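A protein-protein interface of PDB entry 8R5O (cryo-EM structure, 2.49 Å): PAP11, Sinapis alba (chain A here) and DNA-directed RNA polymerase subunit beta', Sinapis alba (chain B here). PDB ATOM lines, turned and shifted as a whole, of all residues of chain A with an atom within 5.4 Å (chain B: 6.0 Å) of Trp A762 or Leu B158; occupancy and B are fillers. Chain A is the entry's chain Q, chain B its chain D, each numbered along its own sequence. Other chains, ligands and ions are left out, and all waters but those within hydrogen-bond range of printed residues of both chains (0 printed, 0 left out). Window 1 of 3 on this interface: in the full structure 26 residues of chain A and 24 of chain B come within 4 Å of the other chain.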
ATOM      1  N   CYS A 703      -0.008  -6.647  32.161  1.00  0.00           N
ATOM      2  CA  CYS A 703      -0.590  -6.284  30.874  1.00  0.00           C
ATOM      3  C   CYS A 703      -0.772  -4.780  30.746  1.00  0.00           C
ATOM      4  O   CYS A 703      -0.750  -4.248  29.631  1.00  0.00           O
ATOM      5  CB  CYS A 703      -1.925  -6.999  30.673  1.00  0.00           C
ATOM      6  SG  CYS A 703      -1.786  -8.761  30.309  1.00  0.00           S
ATOM      7  N   ALA A 706       2.600  -3.354  29.813  1.00  0.00           N
ATOM      8  CA  ALA A 706       2.814  -3.604  28.393  1.00  0.00           C
ATOM      9  C   ALA A 706       1.993  -2.683  27.500  1.00  0.00           C
ATOM     10  O   ALA A 706       2.305  -2.569  26.311  1.00  0.00           O
ATOM     11  CB  ALA A 706       2.494  -5.062  28.064  1.00  0.00           C
ATOM     12  N   MET A 707       0.960  -2.032  28.035  1.00  0.00           N
ATOM     13  CA  MET A 707       0.203  -1.048  27.272  1.00  0.00           C
ATOM     14  C   MET A 707       0.843   0.332  27.291  1.00  0.00           C
ATOM     15  O   MET A 707       0.395   1.214  26.552  1.00  0.00           O
ATOM     16  CB  MET A 707      -1.226  -0.938  27.809  1.00  0.00           C
ATOM     17  CG  MET A 707      -2.073  -2.181  27.617  1.00  0.00           C
ATOM     18  SD  MET A 707      -3.710  -1.997  28.345  1.00  0.00           S
ATOM     19  CE  MET A 707      -4.404  -3.613  28.026  1.00  0.00           C
ATOM     20  N   LEU A 750       8.930  -9.137  24.492  1.00  0.00           N
ATOM     21  CA  LEU A 750       7.558  -9.381  24.059  1.00  0.00           C
ATOM     22  C   LEU A 750       7.229  -8.599  22.794  1.00  0.00           C
ATOM     23  O   LEU A 750       6.519  -9.100  21.915  1.00  0.00           O
ATOM     24  CB  LEU A 750       6.590  -9.016  25.184  1.00  0.00           C
ATOM     25  CG  LEU A 750       5.196  -9.642  25.161  1.00  0.00           C
ATOM     26  CD1 LEU A 750       5.258 -11.091  25.609  1.00  0.00           C
ATOM     27  CD2 LEU A 750       4.249  -8.846  26.038  1.00  0.00           C
ATOM     28  N   ILE A 755       4.340  -9.354  19.019  1.00  0.00           N
ATOM     29  CA  ILE A 755       3.076  -9.243  19.737  1.00  0.00           C
ATOM     30  C   ILE A 755       2.683  -7.777  19.848  1.00  0.00           C
ATOM     31  O   ILE A 755       3.488  -6.934  20.260  1.00  0.00           O
ATOM     32  CB  ILE A 755       3.182  -9.895  21.122  1.00  0.00           C
ATOM     33  CG1 ILE A 755       3.741 -11.310  20.998  1.00  0.00           C
ATOM     34  CG2 ILE A 755       1.825  -9.917  21.801  1.00  0.00           C
ATOM     35  CD1 ILE A 755       3.926 -12.000  22.319  1.00  0.00           C
ATOM     36  N   ASP A 756       1.440  -7.470  19.483  1.00  0.00           N
ATOM     37  CA  ASP A 756       0.884  -6.123  19.594  1.00  0.00           C
ATOM     38  C   ASP A 756       0.074  -6.061  20.885  1.00  0.00           C
ATOM     39  O   ASP A 756      -1.035  -6.597  20.961  1.00  0.00           O
ATOM     40  CB  ASP A 756       0.030  -5.789  18.377  1.00  0.00           C
ATOM     41  CG  ASP A 756      -0.494  -4.367  18.401  1.00  0.00           C
ATOM     42  OD1 ASP A 756      -0.022  -3.564  19.233  1.00  0.00           O
ATOM     43  OD2 ASP A 756      -1.385  -4.051  17.586  1.00  0.00           O
ATOM     44  N   THR A 757       0.629  -5.402  21.901  1.00  0.00           N
ATOM     45  CA  THR A 757       0.001  -5.298  23.212  1.00  0.00           C
ATOM     46  C   THR A 757      -0.581  -3.909  23.459  1.00  0.00           C
ATOM     47  O   THR A 757      -0.641  -3.451  24.601  1.00  0.00           O
ATOM     48  CB  THR A 757       0.998  -5.652  24.313  1.00  0.00           C
ATOM     49  OG1 THR A 757       1.936  -4.581  24.469  1.00  0.00           O
ATOM     50  CG2 THR A 757       1.752  -6.919  23.959  1.00  0.00           C
ATOM     51  N   SER A 758      -1.014  -3.228  22.397  1.00  0.00           N
ATOM     52  CA  SER A 758      -1.554  -1.883  22.543  1.00  0.00           C
ATOM     53  C   SER A 758      -2.872  -1.861  23.306  1.00  0.00           C
ATOM     54  O   SER A 758      -3.220  -0.824  23.880  1.00  0.00           O
ATOM     55  CB  SER A 758      -1.744  -1.239  21.170  1.00  0.00           C
ATOM     56  OG  SER A 758      -2.636  -1.996  20.372  1.00  0.00           O
ATOM     57  N   GLU A 759      -3.602  -2.965  23.329  1.00  0.00           N
ATOM     58  CA  GLU A 759      -4.904  -3.034  23.986  1.00  0.00           C
ATOM     59  C   GLU A 759      -5.267  -4.506  24.153  1.00  0.00           C
ATOM     60  O   GLU A 759      -4.453  -5.397  23.888  1.00  0.00           O
ATOM     61  CB  GLU A 759      -5.967  -2.279  23.189  1.00  0.00           C
ATOM     62  CG  GLU A 759      -6.210  -2.847  21.801  1.00  0.00           C
ATOM     63  CD  GLU A 759      -7.359  -2.169  21.087  1.00  0.00           C
ATOM     64  OE1 GLU A 759      -8.091  -1.396  21.739  1.00  0.00           O
ATOM     65  OE2 GLU A 759      -7.533  -2.410  19.875  1.00  0.00           O
ATOM     66  N   PHE A 760      -6.497  -4.757  24.600  1.00  0.00           N
ATOM     67  CA  PHE A 760      -7.062  -6.096  24.700  1.00  0.00           C
ATOM     68  C   PHE A 760      -7.984  -6.352  23.521  1.00  0.00           C
ATOM     69  O   PHE A 760      -8.803  -5.485  23.187  1.00  0.00           O
ATOM     70  CB  PHE A 760      -7.838  -6.262  26.003  1.00  0.00           C
ATOM     71  CG  PHE A 760      -6.993  -6.696  27.166  1.00  0.00           C
ATOM     72  CD1 PHE A 760      -5.620  -6.807  27.041  1.00  0.00           C
ATOM     73  CD2 PHE A 760      -7.578  -7.011  28.380  1.00  0.00           C
ATOM     74  CE1 PHE A 760      -4.844  -7.211  28.110  1.00  0.00           C
ATOM     75  CE2 PHE A 760      -6.809  -7.418  29.450  1.00  0.00           C
ATOM     76  CZ  PHE A 760      -5.440  -7.517  29.315  1.00  0.00           C
ATOM     77  N   PRO A 761      -7.890  -7.513  22.863  1.00  0.00           N
ATOM     78  CA  PRO A 761      -6.930  -8.601  23.093  1.00  0.00           C
ATOM     79  C   PRO A 761      -5.604  -8.373  22.373  1.00  0.00           C
ATOM     80  O   PRO A 761      -5.540  -7.615  21.410  1.00  0.00           O
ATOM     81  CB  PRO A 761      -7.677  -9.820  22.546  1.00  0.00           C
ATOM     82  CG  PRO A 761      -8.469  -9.261  21.401  1.00  0.00           C
ATOM     83  CD  PRO A 761      -8.891  -7.878  21.845  1.00  0.00           C
ATOM     84  N   TRP A 762      -4.531  -9.017  22.824  1.00  0.00           N
ATOM     85  CA  TRP A 762      -3.254  -8.928  22.132  1.00  0.00           C
ATOM     86  C   TRP A 762      -3.343  -9.574  20.755  1.00  0.00           C
ATOM     87  O   TRP A 762      -4.042 -10.570  20.554  1.00  0.00           O
ATOM     88  CB  TRP A 762      -2.153  -9.607  22.944  1.00  0.00           C
ATOM     89  CG  TRP A 762      -1.784  -8.897  24.202  1.00  0.00           C
ATOM     90  CD1 TRP A 762      -2.326  -7.745  24.685  1.00  0.00           C
ATOM     91  CD2 TRP A 762      -0.779  -9.293  25.142  1.00  0.00           C
ATOM     92  NE1 TRP A 762      -1.724  -7.399  25.869  1.00  0.00           N
ATOM     93  CE2 TRP A 762      -0.771  -8.334  26.171  1.00  0.00           C
ATOM     94  CE3 TRP A 762       0.112 -10.367  25.213  1.00  0.00           C
ATOM     95  CZ2 TRP A 762       0.094  -8.416  27.258  1.00  0.00           C
ATOM     96  CZ3 TRP A 762       0.969 -10.446  26.291  1.00  0.00           C
ATOM     97  CH2 TRP A 762       0.955  -9.477  27.300  1.00  0.00           C
ATOM     98  N   ARG A 763      -2.624  -8.996  19.799  1.00  0.00           N
ATOM     99  CA  ARG A 763      -2.559  -9.524  18.439  1.00  0.00           C
ATOM    100  C   ARG A 763      -1.219 -10.226  18.261  1.00  0.00           C
ATOM    101  O   ARG A 763      -0.184  -9.579  18.089  1.00  0.00           O
ATOM    102  CB  ARG A 763      -2.748  -8.414  17.411  1.00  0.00           C
ATOM    103  CG  ARG A 763      -4.110  -7.754  17.460  1.00  0.00           C
ATOM    104  CD  ARG A 763      -4.403  -7.009  16.172  1.00  0.00           C
ATOM    105  NE  ARG A 763      -5.734  -6.416  16.181  1.00  0.00           N
ATOM    106  CZ  ARG A 763      -6.325  -5.888  15.119  1.00  0.00           C
ATOM    107  NH1 ARG A 763      -5.735  -5.873  13.935  1.00  0.00           N
ATOM    108  NH2 ARG A 763      -7.540  -5.363  15.247  1.00  0.00           N
ATOM    109  N   LEU A 764      -1.241 -11.555  18.307  1.00  0.00           N
ATOM    110  CA  LEU A 764      -0.049 -12.332  18.031  1.00  0.00           C
ATOM    111  C   LEU A 764       0.231 -12.334  16.530  1.00  0.00           C
ATOM    112  O   LEU A 764      -0.673 -12.110  15.721  1.00  0.00           O
ATOM    113  CB  LEU A 764      -0.213 -13.760  18.544  1.00  0.00           C
ATOM    114  CG  LEU A 764      -0.440 -13.930  20.047  1.00  0.00           C
ATOM    115  CD1 LEU A 764      -0.523 -15.400  20.411  1.00  0.00           C
ATOM    116  CD2 LEU A 764       0.659 -13.249  20.836  1.00  0.00           C
ATOM    117  N   SER A 767      -2.063 -14.761  14.594  1.00  0.00           N
ATOM    118  CA  SER A 767      -3.488 -14.598  14.842  1.00  0.00           C
ATOM    119  C   SER A 767      -4.047 -13.538  13.906  1.00  0.00           C
ATOM    120  O   SER A 767      -3.444 -12.476  13.725  1.00  0.00           O
ATOM    121  CB  SER A 767      -3.769 -14.206  16.297  1.00  0.00           C
ATOM    122  OG  SER A 767      -3.422 -12.854  16.536  1.00  0.00           O
ATOM    123  N   ARG B 149      -8.894 -20.557  22.830  1.00  0.00           N
ATOM    124  CA  ARG B 149     -10.117 -20.033  23.428  1.00  0.00           C
ATOM    125  C   ARG B 149     -11.136 -21.142  23.708  1.00  0.00           C
ATOM    126  O   ARG B 149     -12.254 -21.113  23.183  1.00  0.00           O
ATOM    127  CB  ARG B 149     -10.728 -18.952  22.546  1.00  0.00           C
ATOM    128  CG  ARG B 149     -11.667 -18.005  23.276  1.00  0.00           C
ATOM    129  CD  ARG B 149     -10.900 -16.903  23.984  1.00  0.00           C
ATOM    130  NE  ARG B 149     -10.232 -16.018  23.037  1.00  0.00           N
ATOM    131  CZ  ARG B 149     -10.794 -14.951  22.488  1.00  0.00           C
ATOM    132  NH1 ARG B 149     -12.034 -14.596  22.781  1.00  0.00           N
ATOM    133  NH2 ARG B 149     -10.096 -14.223  21.621  1.00  0.00           N
ATOM    134  N   THR B 156     -10.265 -13.304  28.933  1.00  0.00           N
ATOM    135  CA  THR B 156      -9.121 -13.675  28.113  1.00  0.00           C
ATOM    136  C   THR B 156      -8.587 -12.419  27.440  1.00  0.00           C
ATOM    137  O   THR B 156      -9.299 -11.423  27.293  1.00  0.00           O
ATOM    138  CB  THR B 156      -9.483 -14.731  27.058  1.00  0.00           C
ATOM    139  OG1 THR B 156     -10.632 -14.299  26.320  1.00  0.00           O
ATOM    140  CG2 THR B 156      -9.778 -16.073  27.712  1.00  0.00           C
ATOM    141  N   PHE B 157      -7.316 -12.469  27.027  1.00  0.00           N
ATOM    142  CA  PHE B 157      -6.693 -11.280  26.455  1.00  0.00           C
ATOM    143  C   PHE B 157      -5.861 -11.577  25.209  1.00  0.00           C
ATOM    144  O   PHE B 157      -5.047 -10.737  24.809  1.00  0.00           O
ATOM    145  CB  PHE B 157      -5.823 -10.570  27.500  1.00  0.00           C
ATOM    146  CG  PHE B 157      -4.669 -11.392  27.994  1.00  0.00           C
ATOM    147  CD1 PHE B 157      -4.850 -12.335  28.990  1.00  0.00           C
ATOM    148  CD2 PHE B 157      -3.401 -11.210  27.475  1.00  0.00           C
ATOM    149  CE1 PHE B 157      -3.791 -13.090  29.449  1.00  0.00           C
ATOM    150  CE2 PHE B 157      -2.338 -11.961  27.929  1.00  0.00           C
ATOM    151  CZ  PHE B 157      -2.533 -12.901  28.918  1.00  0.00           C
ATOM    152  N   LEU B 158      -6.041 -12.736  24.585  1.00  0.00           N
ATOM    153  CA  LEU B 158      -5.350 -13.076  23.352  1.00  0.00           C
ATOM    154  C   LEU B 158      -6.364 -13.250  22.229  1.00  0.00           C
ATOM    155  O   LEU B 158      -7.474 -13.742  22.448  1.00  0.00           O
ATOM    156  CB  LEU B 158      -4.520 -14.353  23.513  1.00  0.00           C
ATOM    157  CG  LEU B 158      -3.487 -14.343  24.641  1.00  0.00           C
ATOM    158  CD1 LEU B 158      -2.728 -15.656  24.679  1.00  0.00           C
ATOM    159  CD2 LEU B 158      -2.529 -13.173  24.489  1.00  0.00           C
ATOM    160  N   ARG B 159      -5.975 -12.842  21.019  1.00  0.00           N
ATOM    161  CA  ARG B 159      -6.851 -12.912  19.854  1.00  0.00           C
ATOM    162  C   ARG B 159      -6.727 -14.235  19.107  1.00  0.00           C
ATOM    163  O   ARG B 159      -6.996 -14.294  17.901  1.00  0.00           O
ATOM    164  CB  ARG B 159      -6.573 -11.739  18.912  1.00  0.00           C
ATOM    165  CG  ARG B 159      -7.785 -11.282  18.114  1.00  0.00           C
ATOM    166  CD  ARG B 159      -7.482 -10.027  17.320  1.00  0.00           C
ATOM    167  NE  ARG B 159      -8.691  -9.420  16.778  1.00  0.00           N
ATOM    168  CZ  ARG B 159      -9.155  -9.632  15.555  1.00  0.00           C
ATOM    169  NH1 ARG B 159      -8.529 -10.431  14.707  1.00  0.00           N
ATOM    170  NH2 ARG B 159     -10.276  -9.026  15.172  1.00  0.00           N
ATOM    171  N   LEU B 160      -6.317 -15.298  19.791  1.00  0.00           N
ATOM    172  CA  LEU B 160      -6.288 -16.621  19.195  1.00  0.00           C
ATOM    173  C   LEU B 160      -7.682 -17.237  19.204  1.00  0.00           C
ATOM    174  O   LEU B 160      -8.504 -16.952  20.079  1.00  0.00           O
ATOM    175  CB  LEU B 160      -5.317 -17.528  19.950  1.00  0.00           C
ATOM    176  CG  LEU B 160      -3.850 -17.107  20.000  1.00  0.00           C
ATOM    177  CD1 LEU B 160      -3.100 -17.959  21.007  1.00  0.00           C
ATOM    178  CD2 LEU B 160      -3.220 -17.227  18.624  1.00  0.00           C
ATOM    179  N   TRP B 171       3.951 -18.233  22.176  1.00  0.00           N
ATOM    180  CA  TRP B 171       3.377 -18.921  23.325  1.00  0.00           C
ATOM    181  C   TRP B 171       4.365 -19.859  24.005  1.00  0.00           C
ATOM    182  O   TRP B 171       4.108 -20.293  25.133  1.00  0.00           O
ATOM    183  CB  TRP B 171       2.134 -19.694  22.873  1.00  0.00           C
ATOM    184  CG  TRP B 171       1.430 -20.468  23.942  1.00  0.00           C
ATOM    185  CD1 TRP B 171       1.620 -21.780  24.263  1.00  0.00           C
ATOM    186  CD2 TRP B 171       0.407 -19.984  24.817  1.00  0.00           C
ATOM    187  NE1 TRP B 171       0.784 -22.141  25.292  1.00  0.00           N
ATOM    188  CE2 TRP B 171       0.028 -21.056  25.649  1.00  0.00           C
ATOM    189  CE3 TRP B 171      -0.224 -18.747  24.982  1.00  0.00           C
ATOM    190  CZ2 TRP B 171      -0.952 -20.929  26.630  1.00  0.00           C
ATOM    191  CZ3 TRP B 171      -1.196 -18.623  25.955  1.00  0.00           C
ATOM    192  CH2 TRP B 171      -1.551 -19.708  26.768  1.00  0.00           C
ATOM    193  N   ILE B 175       5.610 -15.405  26.195  1.00  0.00           N
ATOM    194  CA  ILE B 175       4.524 -15.257  27.167  1.00  0.00           C
ATOM    195  C   ILE B 175       4.838 -15.934  28.499  1.00  0.00           C
ATOM    196  O   ILE B 175       4.624 -15.306  29.548  1.00  0.00           O
ATOM    197  CB  ILE B 175       3.194 -15.729  26.553  1.00  0.00           C
ATOM    198  CG1 ILE B 175       2.692 -14.725  25.515  1.00  0.00           C
ATOM    199  CG2 ILE B 175       2.142 -15.897  27.627  1.00  0.00           C
ATOM    200  CD1 ILE B 175       3.121 -15.028  24.106  1.00  0.00           C
ATOM    201  N   PHE B 178       7.283 -13.624  30.289  1.00  0.00           N
ATOM    202  CA  PHE B 178       6.773 -12.314  30.681  1.00  0.00           C
ATOM    203  C   PHE B 178       5.914 -12.396  31.937  1.00  0.00           C
ATOM    204  O   PHE B 178       6.018 -11.539  32.821  1.00  0.00           O
ATOM    205  CB  PHE B 178       5.983 -11.702  29.525  1.00  0.00           C
ATOM    206  CG  PHE B 178       5.431 -10.341  29.823  1.00  0.00           C
ATOM    207  CD1 PHE B 178       6.260  -9.234  29.845  1.00  0.00           C
ATOM    208  CD2 PHE B 178       4.081 -10.168  30.069  1.00  0.00           C
ATOM    209  CE1 PHE B 178       5.754  -7.981  30.116  1.00  0.00           C
ATOM    210  CE2 PHE B 178       3.570  -8.918  30.338  1.00  0.00           C
ATOM    211  CZ  PHE B 178       4.407  -7.823  30.363  1.00  0.00           C
ATOM    212  N   PHE B 179       5.060 -13.411  32.034  1.00  0.00           N
ATOM    213  CA  PHE B 179       4.173 -13.575  33.178  1.00  0.00           C
ATOM    214  C   PHE B 179       4.741 -14.493  34.251  1.00  0.00           C
ATOM    215  O   PHE B 179       4.063 -14.729  35.256  1.00  0.00           O
ATOM    216  CB  PHE B 179       2.814 -14.119  32.725  1.00  0.00           C
ATOM    217  CG  PHE B 179       2.024 -13.165  31.875  1.00  0.00           C
ATOM    218  CD1 PHE B 179       1.327 -12.119  32.453  1.00  0.00           C
ATOM    219  CD2 PHE B 179       1.961 -13.328  30.503  1.00  0.00           C
ATOM    220  CE1 PHE B 179       0.594 -11.246  31.675  1.00  0.00           C
ATOM    221  CE2 PHE B 179       1.230 -12.458  29.721  1.00  0.00           C
ATOM    222  CZ  PHE B 179       0.545 -11.417  30.309  1.00  0.00           C
ATOM    223  N   GLU B 191      -6.676 -19.648  27.503  1.00  0.00           N
ATOM    224  CA  GLU B 191      -6.463 -19.074  26.182  1.00  0.00           C
ATOM    225  C   GLU B 191      -6.343 -20.134  25.098  1.00  0.00           C
ATOM    226  O   GLU B 191      -6.903 -19.969  24.010  1.00  0.00           O
ATOM    227  CB  GLU B 191      -5.200 -18.209  26.182  1.00  0.00           C
ATOM    228  CG  GLU B 191      -5.094 -17.261  27.361  1.00  0.00           C
ATOM    229  CD  GLU B 191      -6.021 -16.072  27.243  1.00  0.00           C
ATOM    230  OE1 GLU B 191      -6.539 -15.826  26.136  1.00  0.00           O
ATOM    231  OE2 GLU B 191      -6.228 -15.380  28.261  1.00  0.00           O
ATOM    232  N   ILE B 192      -5.615 -21.213  25.369  1.00  0.00           N
ATOM    233  CA  ILE B 192      -5.467 -22.319  24.428  1.00  0.00           C
ATOM    234  C   ILE B 192      -5.145 -23.580  25.219  1.00  0.00           C
ATOM    235  O   ILE B 192      -4.278 -23.569  26.098  1.00  0.00           O
ATOM    236  CB  ILE B 192      -4.388 -22.028  23.363  1.00  0.00           C
ATOM    237  CG1 ILE B 192      -4.114 -23.264  22.508  1.00  0.00           C
ATOM    238  CG2 ILE B 192      -3.112 -21.525  24.005  1.00  0.00           C
ATOM    239  CD1 ILE B 192      -3.179 -23.001  21.347  1.00  0.00           C
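O of Leu A764 is in hydrogen-bond range of OG of Ser A767 (3.0 Å).
NH2 of Arg B149 lies within hydrogen-bond range of O of Leu B158 (2.8 Å).
The backbone NH (N) of Phe B157 lies within hydrogen-bond range of the side-chain carboxylate (OE2) of Glu B191.
The side-chain carboxylate (OE1) of Glu B191 sits at hydrogen-bond distance from the backbone NH (N) of Leu B158 (3.5 Å).
Among the printed residues, pairs that only touch across the chains: Cys A703 with Phe B179 (3.5 Å), Ile A755 with Ile B175 (3.6 Å), Phe A760 with Phe B157 (3.6 Å), Pro A761 with Phe B157 (3.3 Å), Pro A761 with Leu B158 (3.7 Å), Pro A761 with Arg B159 (3.8 Å), Trp A762 with Leu B158 (3.9 Å), Trp A762 with Phe B179 (3.6 Å), Leu A764 with Leu B160 (3.7 Å), Ser A767 with Arg B159 (3.6 Å) and Ser A767 with Leu B160 (3.9 Å).
Printed residues of chain B within 4 Å of Cys A703: Phe B179.
Of the printed residues of chain B, Ile A755 touches Ile B175.
Ser A758 touches none of the printed residues of chain B.
Printed residues of chain B within 4 Å of Phe A760: Phe B157.
Of chain B, only Phe B157 (2.7 Å), Leu B158 (3.9 Å), Arg B159 (3.0 Å) and Phe B179 (3.6 Å) come within 4 Å of Trp A762.
Of the printed residues of chain B, Leu A764 touches Leu B160 (3.7 Å).
Of chain A, only Pro A761 (3.7 Å) and Trp A762 (3.9 Å) come within 4 Å of Leu B158.
Of the printed residues of chain A, Leu B160 touches Leu A764 (3.7 Å) and Ser A767 (3.9 Å).
The nearest residue of chain A that does not touch Leu B158 is Leu A764 (4.8 Å).
The nearest printed residue of chain B that does not touch Ser A767 is Leu B158 (6.4 Å).
N of Trp A762 is in hydrogen-bond range of O of Phe B157, 2.7 Å away.
O of Trp A762 lies within hydrogen-bond range of N of Arg B159 (3.0 Å).
Hydrophobic or aromatic side chains of chain A within 4 Å of the printed part of chain B: Ile A755, Phe A760, Pro A761, Trp A762 and Leu A764.
Of the 12 printed residues of chain B, 6 touch a printed residue of chain A.
Printed residues of chain B that touch a printed residue of chain A: Phe B157, Leu B158, Arg B159, Leu B160, Ile B175 and Phe B179.
Hydrophobic or aromatic side chains of chain B that line the printed part of chain A: Phe B157, Leu B158, Leu B160, Ile B175 and Phe B179.
Among the printed residues, 13 pairs touch across the chains.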
